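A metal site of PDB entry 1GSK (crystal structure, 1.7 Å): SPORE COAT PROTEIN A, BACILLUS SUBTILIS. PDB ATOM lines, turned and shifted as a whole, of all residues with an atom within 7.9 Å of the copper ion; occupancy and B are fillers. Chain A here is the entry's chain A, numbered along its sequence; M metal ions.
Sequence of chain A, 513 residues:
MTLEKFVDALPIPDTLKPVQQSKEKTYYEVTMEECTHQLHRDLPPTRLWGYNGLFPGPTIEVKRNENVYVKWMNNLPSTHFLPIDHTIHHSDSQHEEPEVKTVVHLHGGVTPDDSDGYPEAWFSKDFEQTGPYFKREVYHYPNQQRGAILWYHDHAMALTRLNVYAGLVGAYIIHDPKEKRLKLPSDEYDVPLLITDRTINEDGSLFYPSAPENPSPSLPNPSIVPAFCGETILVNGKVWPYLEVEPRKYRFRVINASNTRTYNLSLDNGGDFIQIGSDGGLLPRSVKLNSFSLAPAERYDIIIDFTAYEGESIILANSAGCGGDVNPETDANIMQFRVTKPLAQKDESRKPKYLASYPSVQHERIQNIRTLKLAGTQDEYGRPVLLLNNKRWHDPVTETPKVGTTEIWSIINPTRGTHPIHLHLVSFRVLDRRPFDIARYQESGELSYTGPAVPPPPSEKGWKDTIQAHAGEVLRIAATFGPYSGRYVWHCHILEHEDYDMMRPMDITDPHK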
ATOM      1  N   PRO A 226       8.379   8.495  -8.621  1.00  0.00           N
ATOM      2  CA  PRO A 226       9.683   8.894  -9.189  1.00  0.00           C
ATOM      3  C   PRO A 226       9.651   9.295 -10.669  1.00  0.00           C
ATOM      4  O   PRO A 226      10.657   9.793 -11.149  1.00  0.00           O
ATOM      5  CB  PRO A 226      10.558   7.638  -9.032  1.00  0.00           C
ATOM      6  CG  PRO A 226       9.614   6.511  -8.680  1.00  0.00           C
ATOM      7  CD  PRO A 226       8.282   7.049  -8.325  1.00  0.00           C
ATOM      8  N   LEU A 374      25.372  11.949  -9.695  1.00  0.00           N
ATOM      9  CA  LEU A 374      23.919  11.802  -9.603  1.00  0.00           C
ATOM     10  C   LEU A 374      23.655  10.552  -8.774  1.00  0.00           C
ATOM     11  O   LEU A 374      23.948   9.433  -9.188  1.00  0.00           O
ATOM     12  CB  LEU A 374      23.325  11.736 -11.038  1.00  0.00           C
ATOM     13  CG  LEU A 374      23.830  12.841 -11.960  1.00  0.00           C
ATOM     14  CD1 LEU A 374      23.279  12.725 -13.409  1.00  0.00           C
ATOM     15  CD2 LEU A 374      23.561  14.238 -11.417  1.00  0.00           C
ATOM     16  N   LEU A 386      16.264  11.170  -4.801  1.00  0.00           N
ATOM     17  CA  LEU A 386      17.378  11.378  -5.705  1.00  0.00           C
ATOM     18  C   LEU A 386      18.122  12.639  -5.287  1.00  0.00           C
ATOM     19  O   LEU A 386      17.472  13.660  -5.031  1.00  0.00           O
ATOM     20  CB  LEU A 386      16.908  11.566  -7.147  1.00  0.00           C
ATOM     21  CG  LEU A 386      16.580  10.219  -7.800  1.00  0.00           C
ATOM     22  CD1 LEU A 386      15.778  10.439  -9.048  1.00  0.00           C
ATOM     23  CD2 LEU A 386      17.898   9.583  -8.152  1.00  0.00           C
ATOM     24  N   LEU A 388      21.785  15.273  -5.713  1.00  0.00           N
ATOM     25  CA  LEU A 388      22.943  15.734  -6.485  1.00  0.00           C
ATOM     26  C   LEU A 388      24.113  15.669  -5.510  1.00  0.00           C
ATOM     27  O   LEU A 388      24.060  16.314  -4.468  1.00  0.00           O
ATOM     28  CB  LEU A 388      22.709  17.180  -6.951  1.00  0.00           C
ATOM     29  CG  LEU A 388      21.538  17.312  -7.948  1.00  0.00           C
ATOM     30  CD1 LEU A 388      21.242  18.770  -8.308  1.00  0.00           C
ATOM     31  CD2 LEU A 388      21.890  16.520  -9.243  1.00  0.00           C
ATOM     32  N   ASN A 413      27.103  10.014 -13.968  1.00  0.00           N
ATOM     33  CA  ASN A 413      25.809   9.352 -13.814  1.00  0.00           C
ATOM     34  C   ASN A 413      25.891   7.835 -13.739  1.00  0.00           C
ATOM     35  O   ASN A 413      25.929   7.182 -14.778  1.00  0.00           O
ATOM     36  CB  ASN A 413      24.895   9.731 -14.984  1.00  0.00           C
ATOM     37  CG  ASN A 413      23.534   9.134 -14.860  1.00  0.00           C
ATOM     38  OD1 ASN A 413      23.189   8.452 -13.895  1.00  0.00           O
ATOM     39  ND2 ASN A 413      22.699   9.407 -15.868  1.00  0.00           N
ATOM     40  N   THR A 415      23.531   5.994 -12.549  1.00  0.00           N
ATOM     41  CA  THR A 415      22.191   5.441 -12.408  1.00  0.00           C
ATOM     42  C   THR A 415      21.755   4.747 -13.688  1.00  0.00           C
ATOM     43  O   THR A 415      22.463   4.738 -14.651  1.00  0.00           O
ATOM     44  CB  THR A 415      21.183   6.532 -12.037  1.00  0.00           C
ATOM     45  OG1 THR A 415      21.045   7.453 -13.111  1.00  0.00           O
ATOM     46  CG2 THR A 415      21.725   7.394 -10.896  1.00  0.00           C
ATOM     47  N   GLY A 417      19.144   5.459 -15.776  1.00  0.00           N
ATOM     48  CA  GLY A 417      18.571   6.287 -16.841  1.00  0.00           C
ATOM     49  C   GLY A 417      19.253   7.632 -17.057  1.00  0.00           C
ATOM     50  O   GLY A 417      20.184   8.007 -16.346  1.00  0.00           O
ATOM     51  N   THR A 418      18.750   8.379 -18.030  1.00  0.00           N
ATOM     52  CA  THR A 418      19.282   9.711 -18.374  1.00  0.00           C
ATOM     53  C   THR A 418      18.651  10.764 -17.470  1.00  0.00           C
ATOM     54  O   THR A 418      17.482  10.659 -17.118  1.00  0.00           O
ATOM     55  CB  THR A 418      18.911  10.057 -19.835  1.00  0.00           C
ATOM     56  OG1 THR A 418      19.634   9.213 -20.733  1.00  0.00           O
ATOM     57  CG2 THR A 418      19.355  11.480 -20.213  1.00  0.00           C
ATOM     58  N   HIS A 419      19.412  11.808 -17.126  1.00  0.00           N
ATOM     59  CA  HIS A 419      18.832  12.894 -16.330  1.00  0.00           C
ATOM     60  C   HIS A 419      19.135  14.135 -17.096  1.00  0.00           C
ATOM     61  O   HIS A 419      20.294  14.379 -17.436  1.00  0.00           O
ATOM     62  CB  HIS A 419      19.534  12.997 -14.952  1.00  0.00           C
ATOM     63  CG  HIS A 419      19.257  11.837 -14.055  1.00  0.00           C
ATOM     64  ND1 HIS A 419      18.158  11.793 -13.236  1.00  0.00           N
ATOM     65  CD2 HIS A 419      19.908  10.668 -13.867  1.00  0.00           C
ATOM     66  CE1 HIS A 419      18.132  10.663 -12.570  1.00  0.00           C
ATOM     67  NE2 HIS A 419      19.205   9.958 -12.930  1.00  0.00           N
ATOM     68  N   PRO A 420      18.121  14.945 -17.373  1.00  0.00           N
ATOM     69  CA  PRO A 420      18.355  16.205 -18.077  1.00  0.00           C
ATOM     70  C   PRO A 420      18.708  17.293 -17.065  1.00  0.00           C
ATOM     71  O   PRO A 420      17.886  17.680 -16.282  1.00  0.00           O
ATOM     72  CB  PRO A 420      16.986  16.462 -18.784  1.00  0.00           C
ATOM     73  CG  PRO A 420      15.978  15.902 -17.793  1.00  0.00           C
ATOM     74  CD  PRO A 420      16.675  14.680 -17.144  1.00  0.00           C
ATOM     75  N   ILE A 421      19.968  17.731 -17.068  1.00  0.00           N
ATOM     76  CA  ILE A 421      20.433  18.685 -16.050  1.00  0.00           C
ATOM     77  C   ILE A 421      20.368  20.111 -16.551  1.00  0.00           C
ATOM     78  O   ILE A 421      20.839  20.434 -17.613  1.00  0.00           O
ATOM     79  CB  ILE A 421      21.883  18.312 -15.660  1.00  0.00           C
ATOM     80  CG1 ILE A 421      21.975  16.848 -15.219  1.00  0.00           C
ATOM     81  CG2 ILE A 421      22.389  19.306 -14.576  1.00  0.00           C
ATOM     82  CD1 ILE A 421      21.180  16.572 -13.952  1.00  0.00           C
ATOM     83  N   HIS A 491      19.688  21.669 -11.313  1.00  0.00           N
ATOM     84  CA  HIS A 491      18.849  20.531 -10.903  1.00  0.00           C
ATOM     85  C   HIS A 491      18.524  19.656 -12.085  1.00  0.00           C
ATOM     86  O   HIS A 491      18.736  20.039 -13.243  1.00  0.00           O
ATOM     87  CB  HIS A 491      17.497  21.058 -10.339  1.00  0.00           C
ATOM     88  CG  HIS A 491      16.742  21.950 -11.269  1.00  0.00           C
ATOM     89  ND1 HIS A 491      15.671  21.517 -12.025  1.00  0.00           N
ATOM     90  CD2 HIS A 491      16.917  23.259 -11.569  1.00  0.00           C
ATOM     91  CE1 HIS A 491      15.215  22.526 -12.744  1.00  0.00           C
ATOM     92  NE2 HIS A 491      15.931  23.588 -12.472  1.00  0.00           N
ATOM     93  N   CYS A 492      18.029  18.468 -11.772  1.00  0.00           N
ATOM     94  CA  CYS A 492      17.487  17.584 -12.820  1.00  0.00           C
ATOM     95  C   CYS A 492      16.119  18.148 -13.169  1.00  0.00           C
ATOM     96  O   CYS A 492      15.401  18.611 -12.284  1.00  0.00           O
ATOM     97  CB  CYS A 492      17.316  16.222 -12.222  1.00  0.00           C
ATOM     98  SG  CYS A 492      16.551  15.105 -13.440  1.00  0.00           S
ATOM     99  N   HIS A 493      15.775  18.095 -14.472  1.00  0.00           N
ATOM    100  CA  HIS A 493      14.498  18.614 -14.959  1.00  0.00           C
ATOM    101  C   HIS A 493      13.424  17.549 -15.178  1.00  0.00           C
ATOM    102  O   HIS A 493      12.342  17.825 -15.809  1.00  0.00           O
ATOM    103  CB  HIS A 493      14.679  19.523 -16.210  1.00  0.00           C
ATOM    104  CG  HIS A 493      13.745  20.689 -16.186  1.00  0.00           C
ATOM    105  ND1 HIS A 493      12.394  20.560 -16.452  1.00  0.00           N
ATOM    106  CD2 HIS A 493      13.935  21.997 -15.845  1.00  0.00           C
ATOM    107  CE1 HIS A 493      11.812  21.741 -16.314  1.00  0.00           C
ATOM    108  NE2 HIS A 493      12.720  22.628 -15.955  1.00  0.00           N
ATOM    109  N   ILE A 494      13.658  16.354 -14.662  1.00  0.00           N
ATOM    110  CA  ILE A 494      12.537  15.431 -14.493  1.00  0.00           C
ATOM    111  C   ILE A 494      11.876  15.932 -13.213  1.00  0.00           C
ATOM    112  O   ILE A 494      12.468  15.870 -12.113  1.00  0.00           O
ATOM    113  CB  ILE A 494      13.015  13.950 -14.409  1.00  0.00           C
ATOM    114  CG1 ILE A 494      13.545  13.545 -15.779  1.00  0.00           C
ATOM    115  CG2 ILE A 494      11.836  13.030 -13.884  1.00  0.00           C
ATOM    116  CD1 ILE A 494      14.262  12.213 -15.704  1.00  0.00           C
ATOM    117  N   LEU A 495      10.662  16.474 -13.347  1.00  0.00           N
ATOM    118  CA  LEU A 495      10.093  17.180 -12.213  1.00  0.00           C
ATOM    119  C   LEU A 495       9.891  16.318 -10.978  1.00  0.00           C
ATOM    120  O   LEU A 495       9.980  16.801  -9.831  1.00  0.00           O
ATOM    121  CB  LEU A 495       8.785  17.910 -12.644  1.00  0.00           C
ATOM    122  CG  LEU A 495       9.001  18.871 -13.824  1.00  0.00           C
ATOM    123  CD1 LEU A 495       7.682  19.675 -14.045  1.00  0.00           C
ATOM    124  CD2 LEU A 495      10.178  19.830 -13.518  1.00  0.00           C
ATOM    125  N   GLU A 496       9.548  15.040 -11.193  1.00  0.00           N
ATOM    126  CA  GLU A 496       9.366  14.125 -10.109  1.00  0.00           C
ATOM    127  C   GLU A 496      10.703  13.918  -9.338  1.00  0.00           C
ATOM    128  O   GLU A 496      10.677  13.573  -8.157  1.00  0.00           O
ATOM    129  CB  GLU A 496       8.871  12.801 -10.714  1.00  0.00           C
ATOM    130  CG  GLU A 496       7.370  12.819 -11.036  1.00  0.00           C
ATOM    131  CD  GLU A 496       6.982  13.682 -12.231  1.00  0.00           C
ATOM    132  OE1 GLU A 496       7.818  13.914 -13.126  1.00  0.00           O
ATOM    133  OE2 GLU A 496       5.818  14.147 -12.263  1.00  0.00           O
ATOM    134  N   HIS A 497      11.828  14.131 -10.039  1.00  0.00           N
ATOM    135  CA  HIS A 497      13.152  14.010  -9.389  1.00  0.00           C
ATOM    136  C   HIS A 497      13.488  15.305  -8.703  1.00  0.00           C
ATOM    137  O   HIS A 497      13.952  15.302  -7.560  1.00  0.00           O
ATOM    138  CB  HIS A 497      14.237  13.723 -10.421  1.00  0.00           C
ATOM    139  CG  HIS A 497      14.101  12.381 -11.066  1.00  0.00           C
ATOM    140  ND1 HIS A 497      14.978  11.943 -12.047  1.00  0.00           N
ATOM    141  CD2 HIS A 497      13.181  11.412 -10.914  1.00  0.00           C
ATOM    142  CE1 HIS A 497      14.623  10.728 -12.430  1.00  0.00           C
ATOM    143  NE2 HIS A 497      13.533  10.381 -11.743  1.00  0.00           N
ATOM    144  N   GLU A 498      13.253  16.425  -9.398  1.00  0.00           N
ATOM    145  CA  GLU A 498      13.531  17.760  -8.868  1.00  0.00           C
ATOM    146  C   GLU A 498      12.879  18.005  -7.499  1.00  0.00           C
ATOM    147  O   GLU A 498      13.501  18.549  -6.561  1.00  0.00           O
ATOM    148  CB  GLU A 498      13.038  18.798  -9.918  1.00  0.00           C
ATOM    149  CG  GLU A 498      13.092  20.263  -9.462  1.00  0.00           C
ATOM    150  CD  GLU A 498      12.667  21.236 -10.562  1.00  0.00           C
ATOM    151  OE1 GLU A 498      12.719  20.881 -11.755  1.00  0.00           O
ATOM    152  OE2 GLU A 498      12.300  22.383 -10.234  1.00  0.00           O
ATOM    153  N   MET A 502      16.274  16.355  -6.110  1.00  0.00           N
ATOM    154  CA  MET A 502      17.392  16.478  -7.045  1.00  0.00           C
ATOM    155  C   MET A 502      17.623  17.897  -7.575  1.00  0.00           C
ATOM    156  O   MET A 502      17.612  18.186  -8.761  1.00  0.00           O
ATOM    157  CB  MET A 502      17.238  15.431  -8.168  1.00  0.00           C
ATOM    158  CG  MET A 502      18.525  15.110  -8.862  1.00  0.00           C
ATOM    159  SD  MET A 502      18.254  13.707 -10.005  1.00  0.00           S
ATOM    160  CE  MET A 502      19.845  13.599 -10.657  1.00  0.00           C
HETATM  161 CU    CU M   1      16.594  13.022 -12.744  1.00  0.00          CU
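ND1 of His 419 is bound to the copper ion (2.0 Å). The copper ion is bound by ND1 of His 497 (2.1 Å). SG of Cys 492 is bound to the copper ion.
The side-chain hydroxyl (OG1) of Thr 415 is in hydrogen-bond range of a ring nitrogen (NE2) of His 419 (3.1 Å). The side-chain sulfur of Met 502 sits close to a ring nitrogen (ND1) of His 419 (3.8 Å). The backbone NH (N) of Cys 492 is in hydrogen-bond range of the backbone carbonyl oxygen (O) of Met 502. The backbone NH (N) of Met 502 is in hydrogen-bond range of the backbone carbonyl oxygen (O) of His 497, 2.9 Å away. The backbone NH (N) of Met 502 lies within hydrogen-bond range of the backbone carbonyl oxygen (O) of Leu 386 (3.1 Å). A ring nitrogen (NE2) of His 497 sits at hydrogen-bond distance from the backbone carbonyl oxygen (O) of Pro 226 (3.0 Å). The backbone NH (N) of Ile 494 sits close to the side-chain sulfur (SG) of Cys 492.
Ile 494 touches the copper ion (CD1 to CU, 3.9 Å). SD of Met 502 touches the copper ion (3.3 Å).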
